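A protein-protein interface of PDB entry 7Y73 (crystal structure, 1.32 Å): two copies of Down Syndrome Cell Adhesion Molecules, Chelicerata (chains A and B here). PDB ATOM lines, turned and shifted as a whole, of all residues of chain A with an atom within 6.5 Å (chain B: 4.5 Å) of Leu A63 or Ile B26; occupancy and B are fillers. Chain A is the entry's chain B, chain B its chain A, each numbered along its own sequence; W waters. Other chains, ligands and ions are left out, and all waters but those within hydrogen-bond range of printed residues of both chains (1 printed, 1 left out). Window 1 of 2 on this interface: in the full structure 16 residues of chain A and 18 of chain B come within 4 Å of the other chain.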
ATOM      1  N   PHE A  11     -20.648  26.617 -14.306  1.00  0.00           N
ATOM      2  CA  PHE A  11     -21.306  26.735 -15.596  1.00  0.00           C
ATOM      3  C   PHE A  11     -21.987  28.089 -15.703  1.00  0.00           C
ATOM      4  O   PHE A  11     -22.659  28.523 -14.766  1.00  0.00           O
ATOM      5  CB  PHE A  11     -22.354  25.640 -15.803  1.00  0.00           C
ATOM      6  CG  PHE A  11     -23.096  25.785 -17.092  1.00  0.00           C
ATOM      7  CD1 PHE A  11     -24.278  26.508 -17.154  1.00  0.00           C
ATOM      8  CD2 PHE A  11     -22.584  25.244 -18.258  1.00  0.00           C
ATOM      9  CE1 PHE A  11     -24.940  26.670 -18.352  1.00  0.00           C
ATOM     10  CE2 PHE A  11     -23.250  25.394 -19.457  1.00  0.00           C
ATOM     11  CZ  PHE A  11     -24.425  26.111 -19.504  1.00  0.00           C
ATOM     12  N   LYS A  24     -29.274  25.003 -23.311  1.00  0.00           N
ATOM     13  CA  LYS A  24     -29.241  24.103 -22.172  1.00  0.00           C
ATOM     14  C   LYS A  24     -28.264  24.607 -21.124  1.00  0.00           C
ATOM     15  O   LYS A  24     -27.272  25.268 -21.435  1.00  0.00           O
ATOM     16  CB  LYS A  24     -28.790  22.702 -22.581  1.00  0.00           C
ATOM     17  CG  LYS A  24     -29.743  22.003 -23.493  1.00  0.00           C
ATOM     18  CD  LYS A  24     -29.385  20.548 -23.620  1.00  0.00           C
ATOM     19  CE  LYS A  24     -30.387  19.843 -24.502  1.00  0.00           C
ATOM     20  NZ  LYS A  24     -29.885  18.493 -24.856  1.00  0.00           N
ATOM     21  N   ALA A  25     -28.561  24.284 -19.871  1.00  0.00           N
ATOM     22  CA  ALA A  25     -27.621  24.421 -18.775  1.00  0.00           C
ATOM     23  C   ALA A  25     -27.359  23.032 -18.217  1.00  0.00           C
ATOM     24  O   ALA A  25     -28.280  22.213 -18.107  1.00  0.00           O
ATOM     25  CB  ALA A  25     -28.185  25.314 -17.674  1.00  0.00           C
ATOM     26  N   ILE A  26     -26.105  22.757 -17.874  1.00  0.00           N
ATOM     27  CA  ILE A  26     -25.731  21.488 -17.264  1.00  0.00           C
ATOM     28  C   ILE A  26     -25.314  21.744 -15.825  1.00  0.00           C
ATOM     29  O   ILE A  26     -24.480  22.618 -15.552  1.00  0.00           O
ATOM     30  CB  ILE A  26     -24.627  20.759 -18.052  1.00  0.00           C
ATOM     31  CG1 ILE A  26     -24.221  19.486 -17.307  1.00  0.00           C
ATOM     32  CG2 ILE A  26     -23.437  21.662 -18.281  1.00  0.00           C
ATOM     33  CD1 ILE A  26     -23.453  18.505 -18.152  1.00  0.00           C
ATOM     34  N   CYS A  27     -25.907  20.992 -14.909  1.00  0.00           N
ATOM     35  CA  CYS A  27     -25.555  21.029 -13.498  1.00  0.00           C
ATOM     36  C   CYS A  27     -24.946  19.686 -13.135  1.00  0.00           C
ATOM     37  O   CYS A  27     -25.626  18.658 -13.190  1.00  0.00           O
ATOM     38  CB  CYS A  27     -26.797  21.265 -12.656  1.00  0.00           C
ATOM     39  SG  CYS A  27     -26.442  21.525 -10.923  1.00  0.00           S
ATOM     40  N   TRP A  40     -33.735  22.987  -9.735  1.00  0.00           N
ATOM     41  CA  TRP A  40     -33.568  24.170 -10.563  1.00  0.00           C
ATOM     42  C   TRP A  40     -34.538  25.253 -10.117  1.00  0.00           C
ATOM     43  O   TRP A  40     -35.680  24.967  -9.748  1.00  0.00           O
ATOM     44  CB  TRP A  40     -33.824  23.853 -12.036  1.00  0.00           C
ATOM     45  CG  TRP A  40     -32.792  22.970 -12.663  1.00  0.00           C
ATOM     46  CD1 TRP A  40     -32.823  21.612 -12.756  1.00  0.00           C
ATOM     47  CD2 TRP A  40     -31.581  23.391 -13.303  1.00  0.00           C
ATOM     48  NE1 TRP A  40     -31.704  21.158 -13.405  1.00  0.00           N
ATOM     49  CE2 TRP A  40     -30.926  22.230 -13.756  1.00  0.00           C
ATOM     50  CE3 TRP A  40     -30.985  24.635 -13.535  1.00  0.00           C
ATOM     51  CZ2 TRP A  40     -29.708  22.274 -14.431  1.00  0.00           C
ATOM     52  CZ3 TRP A  40     -29.774  24.676 -14.204  1.00  0.00           C
ATOM     53  CH2 TRP A  40     -29.150  23.503 -14.645  1.00  0.00           C
ATOM     54  N   ASP A  54     -37.748  22.022 -20.102  1.00  0.00           N
ATOM     55  CA  ASP A  54     -37.660  20.626 -19.717  1.00  0.00           C
ATOM     56  C   ASP A  54     -36.474  20.448 -18.792  1.00  0.00           C
ATOM     57  O   ASP A  54     -35.440  21.116 -18.947  1.00  0.00           O
ATOM     58  CB  ASP A  54     -37.462  19.772 -20.987  1.00  0.00           C
ATOM     59  CG  ASP A  54     -37.657  18.293 -20.755  1.00  0.00           C
ATOM     60  OD1 ASP A  54     -37.033  17.491 -21.486  1.00  0.00           O
ATOM     61  OD2 ASP A  54     -38.431  17.926 -19.846  1.00  0.00           O
ATOM     62  N   ILE A  55     -36.620  19.538 -17.833  1.00  0.00           N
ATOM     63  CA  ILE A  55     -35.525  19.133 -16.960  1.00  0.00           C
ATOM     64  C   ILE A  55     -35.355  17.628 -17.080  1.00  0.00           C
ATOM     65  O   ILE A  55     -36.312  16.876 -16.873  1.00  0.00           O
ATOM     66  CB  ILE A  55     -35.756  19.526 -15.488  1.00  0.00           C
ATOM     67  CG1 ILE A  55     -35.842  21.041 -15.338  1.00  0.00           C
ATOM     68  CG2 ILE A  55     -34.634  18.958 -14.609  1.00  0.00           C
ATOM     69  CD1 ILE A  55     -36.351  21.477 -13.979  1.00  0.00           C
ATOM     70  N   LYS A  56     -34.137  17.191 -17.400  1.00  0.00           N
ATOM     71  CA  LYS A  56     -33.788  15.776 -17.476  1.00  0.00           C
ATOM     72  C   LYS A  56     -32.667  15.536 -16.478  1.00  0.00           C
ATOM     73  O   LYS A  56     -31.600  16.144 -16.590  1.00  0.00           O
ATOM     74  CB  LYS A  56     -33.327  15.411 -18.888  1.00  0.00           C
ATOM     75  CG  LYS A  56     -34.430  15.531 -19.927  1.00  0.00           C
ATOM     76  CD  LYS A  56     -34.040  14.875 -21.245  1.00  0.00           C
ATOM     77  CE  LYS A  56     -35.244  14.783 -22.176  1.00  0.00           C
ATOM     78  NZ  LYS A  56     -34.854  14.534 -23.593  1.00  0.00           N
ATOM     79  N   THR A  57     -32.903  14.659 -15.505  1.00  0.00           N
ATOM     80  CA  THR A  57     -31.949  14.418 -14.433  1.00  0.00           C
ATOM     81  C   THR A  57     -31.470  12.971 -14.473  1.00  0.00           C
ATOM     82  O   THR A  57     -32.262  12.042 -14.642  1.00  0.00           O
ATOM     83  CB  THR A  57     -32.554  14.773 -13.071  1.00  0.00           C
ATOM     84  OG1 THR A  57     -32.874  16.173 -13.044  1.00  0.00           O
ATOM     85  CG2 THR A  57     -31.569  14.469 -11.955  1.00  0.00           C
ATOM     86  N   PHE A  58     -30.161  12.803 -14.321  1.00  0.00           N
ATOM     87  CA  PHE A  58     -29.464  11.532 -14.396  1.00  0.00           C
ATOM     88  C   PHE A  58     -28.736  11.312 -13.072  1.00  0.00           C
ATOM     89  O   PHE A  58     -28.894  12.079 -12.118  1.00  0.00           O
ATOM     90  CB  PHE A  58     -28.542  11.528 -15.618  1.00  0.00           C
ATOM     91  CG  PHE A  58     -29.267  11.818 -16.901  1.00  0.00           C
ATOM     92  CD1 PHE A  58     -29.734  10.787 -17.697  1.00  0.00           C
ATOM     93  CD2 PHE A  58     -29.516  13.123 -17.290  1.00  0.00           C
ATOM     94  CE1 PHE A  58     -30.419  11.057 -18.866  1.00  0.00           C
ATOM     95  CE2 PHE A  58     -30.203  13.398 -18.452  1.00  0.00           C
ATOM     96  CZ  PHE A  58     -30.650  12.361 -19.245  1.00  0.00           C
ATOM     97  N   TYR A  61     -25.788  14.229 -13.061  1.00  0.00           N
ATOM     98  CA  TYR A  61     -25.913  15.505 -13.743  1.00  0.00           C
ATOM     99  C   TYR A  61     -27.381  15.734 -14.072  1.00  0.00           C
ATOM    100  O   TYR A  61     -28.170  14.788 -14.177  1.00  0.00           O
ATOM    101  CB  TYR A  61     -25.039  15.586 -15.005  1.00  0.00           C
ATOM    102  CG  TYR A  61     -25.217  14.411 -15.927  1.00  0.00           C
ATOM    103  CD1 TYR A  61     -26.071  14.485 -17.021  1.00  0.00           C
ATOM    104  CD2 TYR A  61     -24.554  13.218 -15.694  1.00  0.00           C
ATOM    105  CE1 TYR A  61     -26.248  13.394 -17.865  1.00  0.00           C
ATOM    106  CE2 TYR A  61     -24.726  12.127 -16.524  1.00  0.00           C
ATOM    107  CZ  TYR A  61     -25.577  12.216 -17.607  1.00  0.00           C
ATOM    108  OH  TYR A  61     -25.742  11.127 -18.432  1.00  0.00           O
ATOM    109  N   SER A  62     -27.736  17.000 -14.218  1.00  0.00           N
ATOM    110  CA  SER A  62     -29.084  17.410 -14.565  1.00  0.00           C
ATOM    111  C   SER A  62     -28.995  18.438 -15.680  1.00  0.00           C
ATOM    112  O   SER A  62     -28.125  19.314 -15.656  1.00  0.00           O
ATOM    113  CB  SER A  62     -29.805  18.013 -13.365  1.00  0.00           C
ATOM    114  OG  SER A  62     -31.120  18.395 -13.721  1.00  0.00           O
ATOM    115  N   LEU A  63     -29.886  18.324 -16.658  1.00  0.00           N
ATOM    116  CA  LEU A  63     -29.879  19.184 -17.835  1.00  0.00           C
ATOM    117  C   LEU A  63     -31.193  19.948 -17.899  1.00  0.00           C
ATOM    118  O   LEU A  63     -32.266  19.342 -17.961  1.00  0.00           O
ATOM    119  CB  LEU A  63     -29.689  18.352 -19.103  1.00  0.00           C
ATOM    120  CG  LEU A  63     -28.386  17.554 -19.091  1.00  0.00           C
ATOM    121  CD1 LEU A  63     -28.393  16.488 -20.168  1.00  0.00           C
ATOM    122  CD2 LEU A  63     -27.197  18.484 -19.276  1.00  0.00           C
ATOM    123  N   LEU A  64     -31.100  21.273 -17.880  1.00  0.00           N
ATOM    124  CA  LEU A  64     -32.229  22.158 -18.119  1.00  0.00           C
ATOM    125  C   LEU A  64     -32.200  22.549 -19.588  1.00  0.00           C
ATOM    126  O   LEU A  64     -31.165  23.005 -20.089  1.00  0.00           O
ATOM    127  CB  LEU A  64     -32.109  23.414 -17.255  1.00  0.00           C
ATOM    128  CG  LEU A  64     -33.092  24.549 -17.514  1.00  0.00           C
ATOM    129  CD1 LEU A  64     -34.487  24.130 -17.084  1.00  0.00           C
ATOM    130  CD2 LEU A  64     -32.670  25.814 -16.780  1.00  0.00           C
ATOM    131  N   LYS A  65     -33.330  22.375 -20.273  1.00  0.00           N
ATOM    132  CA  LYS A  65     -33.433  22.665 -21.700  1.00  0.00           C
ATOM    133  C   LYS A  65     -34.547  23.679 -21.921  1.00  0.00           C
ATOM    134  O   LYS A  65     -35.718  23.383 -21.663  1.00  0.00           O
ATOM    135  CB  LYS A  65     -33.703  21.395 -22.513  1.00  0.00           C
ATOM    136  CG  LYS A  65     -33.734  21.640 -24.009  1.00  0.00           C
ATOM    137  CD  LYS A  65     -34.497  20.552 -24.783  1.00  0.00           C
ATOM    138  CE  LYS A  65     -35.818  20.155 -24.133  1.00  0.00           C
ATOM    139  NZ  LYS A  65     -36.752  21.301 -23.969  1.00  0.00           N
ATOM    140  N   PHE B  11     -19.349  25.870 -25.849  1.00  0.00           N
ATOM    141  CA  PHE B  11     -19.007  25.335 -24.540  1.00  0.00           C
ATOM    142  C   PHE B  11     -17.507  25.440 -24.304  1.00  0.00           C
ATOM    143  O   PHE B  11     -16.709  25.142 -25.198  1.00  0.00           O
ATOM    144  CB  PHE B  11     -19.428  23.862 -24.388  1.00  0.00           C
ATOM    145  CG  PHE B  11     -19.148  23.316 -23.029  1.00  0.00           C
ATOM    146  CD1 PHE B  11     -20.090  23.431 -22.025  1.00  0.00           C
ATOM    147  CD2 PHE B  11     -17.923  22.741 -22.733  1.00  0.00           C
ATOM    148  CE1 PHE B  11     -19.828  22.957 -20.762  1.00  0.00           C
ATOM    149  CE2 PHE B  11     -17.652  22.279 -21.471  1.00  0.00           C
ATOM    150  CZ  PHE B  11     -18.607  22.381 -20.484  1.00  0.00           C
ATOM    151  N   LYS B  24     -16.747  17.478 -17.215  1.00  0.00           N
ATOM    152  CA  LYS B  24     -17.612  17.079 -18.312  1.00  0.00           C
ATOM    153  C   LYS B  24     -17.739  18.219 -19.310  1.00  0.00           C
ATOM    154  O   LYS B  24     -17.715  19.397 -18.942  1.00  0.00           O
ATOM    155  CB  LYS B  24     -19.004  16.662 -17.800  1.00  0.00           C
ATOM    156  CG  LYS B  24     -18.941  15.642 -16.663  1.00  0.00           C
ATOM    157  CD  LYS B  24     -20.313  15.104 -16.267  1.00  0.00           C
ATOM    158  CE  LYS B  24     -20.210  14.243 -15.005  1.00  0.00           C
ATOM    159  NZ  LYS B  24     -19.763  15.029 -13.813  1.00  0.00           N
ATOM    160  N   ALA B  25     -17.847  17.853 -20.585  1.00  0.00           N
ATOM    161  CA  ALA B  25     -18.128  18.785 -21.667  1.00  0.00           C
ATOM    162  C   ALA B  25     -19.393  18.322 -22.365  1.00  0.00           C
ATOM    163  O   ALA B  25     -19.534  17.138 -22.681  1.00  0.00           O
ATOM    164  CB  ALA B  25     -16.983  18.830 -22.682  1.00  0.00           C
ATOM    165  N   ILE B  26     -20.311  19.244 -22.604  1.00  0.00           N
ATOM    166  CA  ILE B  26     -21.556  18.935 -23.300  1.00  0.00           C
ATOM    167  C   ILE B  26     -21.459  19.497 -24.713  1.00  0.00           C
ATOM    168  O   ILE B  26     -20.994  20.624 -24.919  1.00  0.00           O
ATOM    169  CB  ILE B  26     -22.811  19.440 -22.558  1.00  0.00           C
ATOM    170  CG1 ILE B  26     -24.071  18.978 -23.299  1.00  0.00           C
ATOM    171  CG2 ILE B  26     -22.781  20.948 -22.391  1.00  0.00           C
ATOM    172  CD1 ILE B  26     -25.359  19.262 -22.557  1.00  0.00           C
ATOM    173  N   CYS B  27     -21.870  18.700 -25.684  1.00  0.00           N
ATOM    174  CA  CYS B  27     -21.895  19.090 -27.088  1.00  0.00           C
ATOM    175  C   CYS B  27     -23.344  18.921 -27.525  1.00  0.00           C
ATOM    176  O   CYS B  27     -23.795  17.804 -27.791  1.00  0.00           O
ATOM    177  CB  CYS B  27     -20.959  18.214 -27.897  1.00  0.00           C
ATOM    178  SG  CYS B  27     -20.869  18.718 -29.610  1.00  0.00           S
ATOM    179  N   THR B  28     -24.079  20.028 -27.582  1.00  0.00           N
ATOM    180  CA  THR B  28     -25.518  20.001 -27.743  1.00  0.00           C
ATOM    181  C   THR B  28     -25.931  21.055 -28.759  1.00  0.00           C
ATOM    182  O   THR B  28     -25.347  22.152 -28.792  1.00  0.00           O
ATOM    183  CB  THR B  28     -26.186  20.241 -26.375  1.00  0.00           C
ATOM    184  OG1 THR B  28     -27.583  19.941 -26.452  1.00  0.00           O
ATOM    185  CG2 THR B  28     -25.967  21.663 -25.877  1.00  0.00           C
ATOM    186  N   TYR B  61     -27.572  14.742 -28.694  1.00  0.00           N
ATOM    187  CA  TYR B  61     -26.435  15.469 -28.141  1.00  0.00           C
ATOM    188  C   TYR B  61     -25.447  14.455 -27.581  1.00  0.00           C
ATOM    189  O   TYR B  61     -25.710  13.251 -27.558  1.00  0.00           O
ATOM    190  CB  TYR B  61     -26.846  16.510 -27.088  1.00  0.00           C
ATOM    191  CG  TYR B  61     -27.656  16.012 -25.910  1.00  0.00           C
ATOM    192  CD1 TYR B  61     -27.085  15.890 -24.652  1.00  0.00           C
ATOM    193  CD2 TYR B  61     -29.011  15.722 -26.044  1.00  0.00           C
ATOM    194  CE1 TYR B  61     -27.832  15.467 -23.563  1.00  0.00           C
ATOM    195  CE2 TYR B  61     -29.761  15.292 -24.965  1.00  0.00           C
ATOM    196  CZ  TYR B  61     -29.167  15.166 -23.728  1.00  0.00           C
ATOM    197  OH  TYR B  61     -29.916  14.745 -22.652  1.00  0.00           O
ATOM    198  N   SER B  62     -24.296  14.961 -27.133  1.00  0.00           N
ATOM    199  CA  SER B  62     -23.197  14.123 -26.668  1.00  0.00           C
ATOM    200  C   SER B  62     -22.565  14.768 -25.443  1.00  0.00           C
ATOM    201  O   SER B  62     -22.532  15.993 -25.323  1.00  0.00           O
ATOM    202  CB  SER B  62     -22.138  13.949 -27.770  1.00  0.00           C
ATOM    203  OG  SER B  62     -21.101  13.073 -27.373  1.00  0.00           O
ATOM    204  N   PHE B  90     -16.844  23.202 -32.060  1.00  0.00           N
ATOM    205  CA  PHE B  90     -16.126  24.056 -31.123  1.00  0.00           C
ATOM    206  C   PHE B  90     -14.940  23.273 -30.568  1.00  0.00           C
ATOM    207  O   PHE B  90     -14.916  22.040 -30.598  1.00  0.00           O
ATOM    208  CB  PHE B  90     -17.024  24.607 -29.990  1.00  0.00           C
ATOM    209  CG  PHE B  90     -17.569  23.554 -29.068  1.00  0.00           C
ATOM    210  CD1 PHE B  90     -16.793  23.029 -28.051  1.00  0.00           C
ATOM    211  CD2 PHE B  90     -18.863  23.100 -29.210  1.00  0.00           C
ATOM    212  CE1 PHE B  90     -17.296  22.056 -27.206  1.00  0.00           C
ATOM    213  CE2 PHE B  90     -19.371  22.135 -28.370  1.00  0.00           C
ATOM    214  CZ  PHE B  90     -18.590  21.617 -27.362  1.00  0.00           C
HETATM  215  O   HOH W   1     -31.104  17.572 -22.612  1.00  0.00           O
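OG1 of Thr B28 sits at hydrogen-bond distance from NZ of Lys A24 (3.2 Å).
The backbone NH (N) of Leu A63 lies within hydrogen-bond range of the backbone carbonyl oxygen (O) of Lys A56 (2.8 Å).
Among the printed residues, merely in contact across the chains: Lys A24 with Tyr B61 (3.1 Å), Leu A63 with Tyr B61 (3.4 Å) and Leu A63 with Ile B26 (3.8 Å).
Of the printed residues of chain B, Lys A24 touches Thr B28 (3.2 Å) and Tyr B61 (3.1 Å).
Ala A25 touches none of the printed residues of chain B.
Of chain B, only Ile B26 and Tyr B61 come within 4 Å of Leu A63.
Printed residues of chain A within 4 Å of Thr B28: Lys A24 (3.2 Å).
Of the printed residues of chain A, Tyr B61 touches Lys A24 (3.1 Å) and Leu A63 (3.4 Å).
The nearest printed residue of chain B that does not touch Leu A63 is Thr B28 (7.2 Å).
The nearest printed residue of chain A that does not touch Thr B28 is Lys A65 (6.8 Å).
Hydrophobic or aromatic side chains of chain A that line the printed part of chain B: Leu A63.
Along chain B the printed residues that touch a printed residue of chain A span positions 26 to 61.
Among the printed residues, no Asp or Glu carboxylate lies within 4 Å of a Lys or Arg side-chain nitrogen of the other chain.
Lys A24 touches Tyr B61, but with the chains exchanged Tyr A61 does not touch Lys B24 (4.5 Å).
Water W1 lies within hydrogen-bond range of NZ of Lys A24 (2.7 Å) and OH of Tyr B61 (3.1 Å).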
